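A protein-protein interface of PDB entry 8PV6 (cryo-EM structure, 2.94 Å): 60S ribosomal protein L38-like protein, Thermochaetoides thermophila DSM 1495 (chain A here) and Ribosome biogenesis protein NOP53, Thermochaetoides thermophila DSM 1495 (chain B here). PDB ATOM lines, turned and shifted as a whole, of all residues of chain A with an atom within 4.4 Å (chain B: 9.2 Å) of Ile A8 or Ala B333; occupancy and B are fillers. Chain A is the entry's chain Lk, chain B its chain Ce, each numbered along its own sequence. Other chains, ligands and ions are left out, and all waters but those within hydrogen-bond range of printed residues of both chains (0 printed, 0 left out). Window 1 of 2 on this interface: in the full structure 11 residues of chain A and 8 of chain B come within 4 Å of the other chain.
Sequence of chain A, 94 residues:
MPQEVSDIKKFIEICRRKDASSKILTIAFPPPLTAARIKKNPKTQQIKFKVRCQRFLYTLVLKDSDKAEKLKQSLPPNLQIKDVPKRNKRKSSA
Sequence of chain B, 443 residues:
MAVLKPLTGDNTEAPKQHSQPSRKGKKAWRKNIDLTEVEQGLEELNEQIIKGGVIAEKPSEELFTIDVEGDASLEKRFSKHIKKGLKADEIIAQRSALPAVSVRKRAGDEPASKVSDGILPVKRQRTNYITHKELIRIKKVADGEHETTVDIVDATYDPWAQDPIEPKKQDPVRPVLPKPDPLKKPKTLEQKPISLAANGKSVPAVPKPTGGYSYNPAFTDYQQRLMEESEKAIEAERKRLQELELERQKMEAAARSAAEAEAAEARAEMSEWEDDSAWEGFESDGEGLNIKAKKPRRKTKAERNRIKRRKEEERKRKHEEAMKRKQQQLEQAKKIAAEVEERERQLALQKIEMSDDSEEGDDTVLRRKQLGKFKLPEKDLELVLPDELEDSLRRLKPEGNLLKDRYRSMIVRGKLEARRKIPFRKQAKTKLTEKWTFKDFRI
Among the printed residues, merely in contact across the chains: Ile A8 with Gln B329 (3.2 Å), Ile A8 with Leu B330 (3.6 Å), Ile A12 with Val B340 (3.7 Å), Lys A9 with Ile B336 (3.7 Å), Ser A6 with Lys B326 (3.7 Å) and Ile A8 with Ala B333 (3.9 Å).
OD1 of Asp A7 sits close to OE1 of Gln B329 (2.9 Å).
Printed residues of chain B within 4 Å of Ile A8: Gln B329, Leu B330 and Ala B333.
Asp A7 touches just one residue of chain B: Gln B329.
Printed residues of chain B within 4 Å of Ser A6: Lys B326.
Of the printed residues of chain A, Gln B329 touches Asp A7 (2.9 Å) and Ile A8 (3.2 Å).
Glu B331 touches none of the printed residues of chain A.
Lys B334 touches none of the printed residues of chain A.
The nearest residue of chain A that does not touch Ala B333 is Ile A12 (4.3 Å).
Printed residues of chain A that touch a printed residue of chain B: Ser A6, Asp A7, Ile A8, Lys A9 and Ile A12.
Hydrophobic or aromatic side chains of chain A that line the printed part of chain B: Ile A8 and Ile A12.
Of the 16 printed residues of chain B, 6 touch a printed residue of chain A.
Along chain B the printed residues that touch a printed residue of chain A span positions 326 to 340.
The side-chain carboxylate of Asp A7 lies close to the backbone NH of Lys A9, at 3.4 Å.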
ATOM      1  N   SER A   6      -7.004  15.335  20.608  1.00  0.00           N
ATOM      2  CA  SER A   6      -6.906  14.008  20.017  1.00  0.00           C
ATOM      3  C   SER A   6      -7.249  13.988  18.537  1.00  0.00           C
ATOM      4  O   SER A   6      -7.262  12.910  17.934  1.00  0.00           O
ATOM      5  CB  SER A   6      -7.815  13.026  20.761  1.00  0.00           C
ATOM      6  OG  SER A   6      -7.494  12.979  22.137  1.00  0.00           O
ATOM      7  N   ASP A   7      -7.537  15.138  17.938  1.00  0.00           N
ATOM      8  CA  ASP A   7      -7.816  15.235  16.514  1.00  0.00           C
ATOM      9  C   ASP A   7      -6.840  16.223  15.895  1.00  0.00           C
ATOM     10  O   ASP A   7      -6.819  17.400  16.273  1.00  0.00           O
ATOM     11  CB  ASP A   7      -9.258  15.682  16.264  1.00  0.00           C
ATOM     12  CG  ASP A   7      -9.791  15.214  14.923  1.00  0.00           C
ATOM     13  OD1 ASP A   7      -8.980  14.958  14.008  1.00  0.00           O
ATOM     14  OD2 ASP A   7     -11.026  15.099  14.784  1.00  0.00           O
ATOM     15  N   ILE A   8      -6.050  15.753  14.926  1.00  0.00           N
ATOM     16  CA  ILE A   8      -5.011  16.611  14.367  1.00  0.00           C
ATOM     17  C   ILE A   8      -5.630  17.686  13.489  1.00  0.00           C
ATOM     18  O   ILE A   8      -5.026  18.740  13.258  1.00  0.00           O
ATOM     19  CB  ILE A   8      -3.977  15.789  13.587  1.00  0.00           C
ATOM     20  CG1 ILE A   8      -4.653  15.006  12.478  1.00  0.00           C
ATOM     21  CG2 ILE A   8      -3.284  14.820  14.513  1.00  0.00           C
ATOM     22  CD1 ILE A   8      -3.670  14.335  11.594  1.00  0.00           C
ATOM     23  N   LYS A   9      -6.850  17.447  12.999  1.00  0.00           N
ATOM     24  CA  LYS A   9      -7.604  18.513  12.350  1.00  0.00           C
ATOM     25  C   LYS A   9      -7.829  19.667  13.311  1.00  0.00           C
ATOM     26  O   LYS A   9      -7.452  20.811  13.021  1.00  0.00           O
ATOM     27  CB  LYS A   9      -8.943  17.983  11.841  1.00  0.00           C
ATOM     28  CG  LYS A   9      -9.765  19.034  11.109  1.00  0.00           C
ATOM     29  CD  LYS A   9     -11.004  18.440  10.471  1.00  0.00           C
ATOM     30  CE  LYS A   9     -11.772  19.497   9.709  1.00  0.00           C
ATOM     31  NZ  LYS A   9     -12.990  18.944   9.060  1.00  0.00           N
ATOM     32  N   LYS A  10      -8.364  19.360  14.498  1.00  0.00           N
ATOM     33  CA  LYS A  10      -8.584  20.373  15.522  1.00  0.00           C
ATOM     34  C   LYS A  10      -7.275  21.036  15.921  1.00  0.00           C
ATOM     35  O   LYS A  10      -7.234  22.245  16.176  1.00  0.00           O
ATOM     36  CB  LYS A  10      -9.249  19.741  16.740  1.00  0.00           C
ATOM     37  CG  LYS A  10     -10.687  19.319  16.518  1.00  0.00           C
ATOM     38  CD  LYS A  10     -11.255  18.650  17.760  1.00  0.00           C
ATOM     39  CE  LYS A  10     -11.408  19.653  18.894  1.00  0.00           C
ATOM     40  NZ  LYS A  10     -12.441  20.685  18.592  1.00  0.00           N
ATOM     41  N   PHE A  11      -6.188  20.261  15.945  1.00  0.00           N
ATOM     42  CA  PHE A  11      -4.870  20.833  16.198  1.00  0.00           C
ATOM     43  C   PHE A  11      -4.474  21.821  15.106  1.00  0.00           C
ATOM     44  O   PHE A  11      -3.813  22.827  15.381  1.00  0.00           O
ATOM     45  CB  PHE A  11      -3.837  19.716  16.329  1.00  0.00           C
ATOM     46  CG  PHE A  11      -2.550  20.155  16.956  1.00  0.00           C
ATOM     47  CD1 PHE A  11      -2.480  20.392  18.319  1.00  0.00           C
ATOM     48  CD2 PHE A  11      -1.405  20.307  16.193  1.00  0.00           C
ATOM     49  CE1 PHE A  11      -1.300  20.792  18.907  1.00  0.00           C
ATOM     50  CE2 PHE A  11      -0.215  20.698  16.780  1.00  0.00           C
ATOM     51  CZ  PHE A  11      -0.167  20.949  18.137  1.00  0.00           C
ATOM     52  N   ILE A  12      -4.886  21.563  13.864  1.00  0.00           N
ATOM     53  CA  ILE A  12      -4.567  22.475  12.766  1.00  0.00           C
ATOM     54  C   ILE A  12      -5.346  23.785  12.892  1.00  0.00           C
ATOM     55  O   ILE A  12      -4.770  24.870  12.723  1.00  0.00           O
ATOM     56  CB  ILE A  12      -4.796  21.788  11.408  1.00  0.00           C
ATOM     57  CG1 ILE A  12      -3.707  20.750  11.171  1.00  0.00           C
ATOM     58  CG2 ILE A  12      -4.757  22.787  10.277  1.00  0.00           C
ATOM     59  CD1 ILE A  12      -3.896  19.972   9.903  1.00  0.00           C
ATOM     60  N   LEU A  60      -0.664  17.614  21.579  1.00  0.00           N
ATOM     61  CA  LEU A  60      -1.029  16.495  20.722  1.00  0.00           C
ATOM     62  C   LEU A  60       0.047  15.429  20.878  1.00  0.00           C
ATOM     63  O   LEU A  60       1.226  15.689  20.615  1.00  0.00           O
ATOM     64  CB  LEU A  60      -1.157  16.953  19.272  1.00  0.00           C
ATOM     65  CG  LEU A  60      -1.191  15.896  18.173  1.00  0.00           C
ATOM     66  CD1 LEU A  60      -2.498  15.125  18.206  1.00  0.00           C
ATOM     67  CD2 LEU A  60      -0.982  16.556  16.827  1.00  0.00           C
ATOM     68  N   LEU A  71       3.755  16.484   9.596  1.00  0.00           N
ATOM     69  CA  LEU A  71       2.811  17.366  10.277  1.00  0.00           C
ATOM     70  C   LEU A  71       3.480  18.672  10.687  1.00  0.00           C
ATOM     71  O   LEU A  71       2.849  19.737  10.663  1.00  0.00           O
ATOM     72  CB  LEU A  71       2.223  16.658  11.498  1.00  0.00           C
ATOM     73  CG  LEU A  71       1.158  17.417  12.289  1.00  0.00           C
ATOM     74  CD1 LEU A  71      -0.030  17.756  11.405  1.00  0.00           C
ATOM     75  CD2 LEU A  71       0.719  16.611  13.493  1.00  0.00           C
ATOM     76  N   ARG B 325      -7.623   5.380  14.510  1.00  0.00           N
ATOM     77  CA  ARG B 325      -8.211   6.503  13.777  1.00  0.00           C
ATOM     78  C   ARG B 325      -7.287   7.713  13.783  1.00  0.00           C
ATOM     79  O   ARG B 325      -7.133   8.392  12.755  1.00  0.00           O
ATOM     80  CB  ARG B 325      -9.574   6.900  14.341  1.00  0.00           C
ATOM     81  CG  ARG B 325     -10.674   5.889  14.131  1.00  0.00           C
ATOM     82  CD  ARG B 325     -12.001   6.424  14.654  1.00  0.00           C
ATOM     83  NE  ARG B 325     -12.042   6.539  16.106  1.00  0.00           N
ATOM     84  CZ  ARG B 325     -12.109   7.688  16.764  1.00  0.00           C
ATOM     85  NH1 ARG B 325     -12.150   8.849  16.130  1.00  0.00           N
ATOM     86  NH2 ARG B 325     -12.142   7.673  18.094  1.00  0.00           N
ATOM     87  N   LYS B 326      -6.667   8.001  14.930  1.00  0.00           N
ATOM     88  CA  LYS B 326      -5.692   9.084  14.982  1.00  0.00           C
ATOM     89  C   LYS B 326      -4.506   8.801  14.064  1.00  0.00           C
ATOM     90  O   LYS B 326      -3.994   9.710  13.406  1.00  0.00           O
ATOM     91  CB  LYS B 326      -5.226   9.310  16.422  1.00  0.00           C
ATOM     92  CG  LYS B 326      -4.237  10.456  16.589  1.00  0.00           C
ATOM     93  CD  LYS B 326      -4.154  10.932  18.034  1.00  0.00           C
ATOM     94  CE  LYS B 326      -3.729   9.813  18.972  1.00  0.00           C
ATOM     95  NZ  LYS B 326      -3.678  10.265  20.390  1.00  0.00           N
ATOM     96  N   GLN B 327      -4.081   7.536  13.979  1.00  0.00           N
ATOM     97  CA  GLN B 327      -2.967   7.174  13.101  1.00  0.00           C
ATOM     98  C   GLN B 327      -3.319   7.328  11.623  1.00  0.00           C
ATOM     99  O   GLN B 327      -2.483   7.760  10.819  1.00  0.00           O
ATOM    100  CB  GLN B 327      -2.520   5.741  13.389  1.00  0.00           C
ATOM    101  CG  GLN B 327      -1.306   5.284  12.593  1.00  0.00           C
ATOM    102  CD  GLN B 327      -0.031   6.000  12.982  1.00  0.00           C
ATOM    103  OE1 GLN B 327       0.090   6.527  14.088  1.00  0.00           O
ATOM    104  NE2 GLN B 327       0.932   6.028  12.068  1.00  0.00           N
ATOM    105  N   GLN B 328      -4.537   6.952  11.229  1.00  0.00           N
ATOM    106  CA  GLN B 328      -4.885   7.075   9.816  1.00  0.00           C
ATOM    107  C   GLN B 328      -5.084   8.539   9.432  1.00  0.00           C
ATOM    108  O   GLN B 328      -4.743   8.951   8.314  1.00  0.00           O
ATOM    109  CB  GLN B 328      -6.101   6.209   9.472  1.00  0.00           C
ATOM    110  CG  GLN B 328      -7.433   6.527  10.136  1.00  0.00           C
ATOM    111  CD  GLN B 328      -8.212   7.614   9.413  1.00  0.00           C
ATOM    112  OE1 GLN B 328      -8.096   7.767   8.197  1.00  0.00           O
ATOM    113  NE2 GLN B 328      -9.039   8.351  10.152  1.00  0.00           N
ATOM    114  N   GLN B 329      -5.614   9.353  10.355  1.00  0.00           N
ATOM    115  CA  GLN B 329      -5.610  10.798  10.125  1.00  0.00           C
ATOM    116  C   GLN B 329      -4.187  11.332  10.018  1.00  0.00           C
ATOM    117  O   GLN B 329      -3.898  12.188   9.173  1.00  0.00           O
ATOM    118  CB  GLN B 329      -6.361  11.531  11.237  1.00  0.00           C
ATOM    119  CG  GLN B 329      -7.853  11.272  11.285  1.00  0.00           C
ATOM    120  CD  GLN B 329      -8.494  11.857  12.526  1.00  0.00           C
ATOM    121  OE1 GLN B 329      -7.805  12.323  13.432  1.00  0.00           O
ATOM    122  NE2 GLN B 329      -9.820  11.820  12.581  1.00  0.00           N
ATOM    123  N   LEU B 330      -3.289  10.833  10.874  1.00  0.00           N
ATOM    124  CA  LEU B 330      -1.880  11.213  10.847  1.00  0.00           C
ATOM    125  C   LEU B 330      -1.246  10.904   9.498  1.00  0.00           C
ATOM    126  O   LEU B 330      -0.412  11.670   9.001  1.00  0.00           O
ATOM    127  CB  LEU B 330      -1.164  10.488  11.993  1.00  0.00           C
ATOM    128  CG  LEU B 330       0.275  10.688  12.452  1.00  0.00           C
ATOM    129  CD1 LEU B 330       0.359  10.328  13.911  1.00  0.00           C
ATOM    130  CD2 LEU B 330       1.157   9.741  11.696  1.00  0.00           C
ATOM    131  N   GLU B 331      -1.630   9.782   8.891  1.00  0.00           N
ATOM    132  CA  GLU B 331      -1.191   9.489   7.531  1.00  0.00           C
ATOM    133  C   GLU B 331      -1.831  10.413   6.499  1.00  0.00           C
ATOM    134  O   GLU B 331      -1.173  10.770   5.517  1.00  0.00           O
ATOM    135  CB  GLU B 331      -1.491   8.029   7.188  1.00  0.00           C
ATOM    136  CG  GLU B 331      -0.588   7.034   7.901  1.00  0.00           C
ATOM    137  CD  GLU B 331       0.847   7.085   7.407  1.00  0.00           C
ATOM    138  OE1 GLU B 331       1.061   7.385   6.213  1.00  0.00           O
ATOM    139  OE2 GLU B 331       1.765   6.843   8.218  1.00  0.00           O
ATOM    140  N   GLN B 332      -3.092  10.803   6.697  1.00  0.00           N
ATOM    141  CA  GLN B 332      -3.803  11.674   5.765  1.00  0.00           C
ATOM    142  C   GLN B 332      -3.848  13.127   6.239  1.00  0.00           C
ATOM    143  O   GLN B 332      -4.856  13.814   6.052  1.00  0.00           O
ATOM    144  CB  GLN B 332      -5.220  11.155   5.532  1.00  0.00           C
ATOM    145  CG  GLN B 332      -5.276   9.796   4.870  1.00  0.00           C
ATOM    146  CD  GLN B 332      -4.745   9.823   3.453  1.00  0.00           C
ATOM    147  OE1 GLN B 332      -4.976  10.775   2.709  1.00  0.00           O
ATOM    148  NE2 GLN B 332      -4.029   8.773   3.071  1.00  0.00           N
ATOM    149  N   ALA B 333      -2.767  13.597   6.866  1.00  0.00           N
ATOM    150  CA  ALA B 333      -2.764  14.912   7.506  1.00  0.00           C
ATOM    151  C   ALA B 333      -2.813  16.065   6.503  1.00  0.00           C
ATOM    152  O   ALA B 333      -3.400  17.113   6.794  1.00  0.00           O
ATOM    153  CB  ALA B 333      -1.533  15.045   8.401  1.00  0.00           C
ATOM    154  N   LYS B 334      -2.178  15.912   5.335  1.00  0.00           N
ATOM    155  CA  LYS B 334      -1.999  17.049   4.426  1.00  0.00           C
ATOM    156  C   LYS B 334      -3.321  17.507   3.811  1.00  0.00           C
ATOM    157  O   LYS B 334      -3.587  18.716   3.711  1.00  0.00           O
ATOM    158  CB  LYS B 334      -1.002  16.689   3.324  1.00  0.00           C
ATOM    159  CG  LYS B 334       0.426  16.496   3.806  1.00  0.00           C
ATOM    160  CD  LYS B 334       1.389  16.418   2.634  1.00  0.00           C
ATOM    161  CE  LYS B 334       2.832  16.331   3.105  1.00  0.00           C
ATOM    162  NZ  LYS B 334       3.785  16.317   1.961  1.00  0.00           N
ATOM    163  N   LYS B 335      -4.162  16.558   3.396  1.00  0.00           N
ATOM    164  CA  LYS B 335      -5.432  16.921   2.775  1.00  0.00           C
ATOM    165  C   LYS B 335      -6.373  17.558   3.790  1.00  0.00           C
ATOM    166  O   LYS B 335      -7.256  18.338   3.425  1.00  0.00           O
ATOM    167  CB  LYS B 335      -6.067  15.695   2.116  1.00  0.00           C
ATOM    168  CG  LYS B 335      -6.598  14.642   3.074  1.00  0.00           C
ATOM    169  CD  LYS B 335      -7.240  13.494   2.311  1.00  0.00           C
ATOM    170  CE  LYS B 335      -7.853  12.473   3.255  1.00  0.00           C
ATOM    171  NZ  LYS B 335      -8.488  11.347   2.517  1.00  0.00           N
ATOM    172  N   ILE B 336      -6.172  17.263   5.078  1.00  0.00           N
ATOM    173  CA  ILE B 336      -6.918  17.938   6.136  1.00  0.00           C
ATOM    174  C   ILE B 336      -6.575  19.425   6.166  1.00  0.00           C
ATOM    175  O   ILE B 336      -7.462  20.284   6.292  1.00  0.00           O
ATOM    176  CB  ILE B 336      -6.637  17.258   7.488  1.00  0.00           C
ATOM    177  CG1 ILE B 336      -7.228  15.847   7.510  1.00  0.00           C
ATOM    178  CG2 ILE B 336      -7.183  18.079   8.629  1.00  0.00           C
ATOM    179  CD1 ILE B 336      -6.899  15.071   8.762  1.00  0.00           C
ATOM    180  N   ALA B 337      -5.284  19.749   6.042  1.00  0.00           N
ATOM    181  CA  ALA B 337      -4.865  21.145   5.956  1.00  0.00           C
ATOM    182  C   ALA B 337      -5.419  21.810   4.704  1.00  0.00           C
ATOM    183  O   ALA B 337      -5.825  22.980   4.741  1.00  0.00           O
ATOM    184  CB  ALA B 337      -3.340  21.239   5.983  1.00  0.00           C
ATOM    185  N   ALA B 338      -5.455  21.073   3.587  1.00  0.00           N
ATOM    186  CA  ALA B 338      -6.058  21.614   2.371  1.00  0.00           C
ATOM    187  C   ALA B 338      -7.540  21.930   2.573  1.00  0.00           C
ATOM    188  O   ALA B 338      -8.016  22.998   2.167  1.00  0.00           O
ATOM    189  CB  ALA B 338      -5.872  20.636   1.211  1.00  0.00           C
ATOM    190  N   GLU B 339      -8.273  21.022   3.230  1.00  0.00           N
ATOM    191  CA  GLU B 339      -9.700  21.235   3.466  1.00  0.00           C
ATOM    192  C   GLU B 339      -9.955  22.405   4.405  1.00  0.00           C
ATOM    193  O   GLU B 339     -10.893  23.180   4.190  1.00  0.00           O
ATOM    194  CB  GLU B 339     -10.355  19.970   4.022  1.00  0.00           C
ATOM    195  CG  GLU B 339     -10.388  18.800   3.063  1.00  0.00           C
ATOM    196  CD  GLU B 339     -10.444  17.469   3.781  1.00  0.00           C
ATOM    197  OE1 GLU B 339     -10.364  17.461   5.027  1.00  0.00           O
ATOM    198  OE2 GLU B 339     -10.560  16.430   3.097  1.00  0.00           O
ATOM    199  N   VAL B 340      -9.149  22.546   5.462  1.00  0.00           N
ATOM    200  CA  VAL B 340      -9.398  23.638   6.403  1.00  0.00           C
ATOM    201  C   VAL B 340      -9.027  24.977   5.769  1.00  0.00           C
ATOM    202  O   VAL B 340      -9.678  26.001   6.019  1.00  0.00           O
ATOM    203  CB  VAL B 340      -8.678  23.399   7.746  1.00  0.00           C
ATOM    204  CG1 VAL B 340      -7.172  23.476   7.626  1.00  0.00           C
ATOM    205  CG2 VAL B 340      -9.183  24.371   8.806  1.00  0.00           C
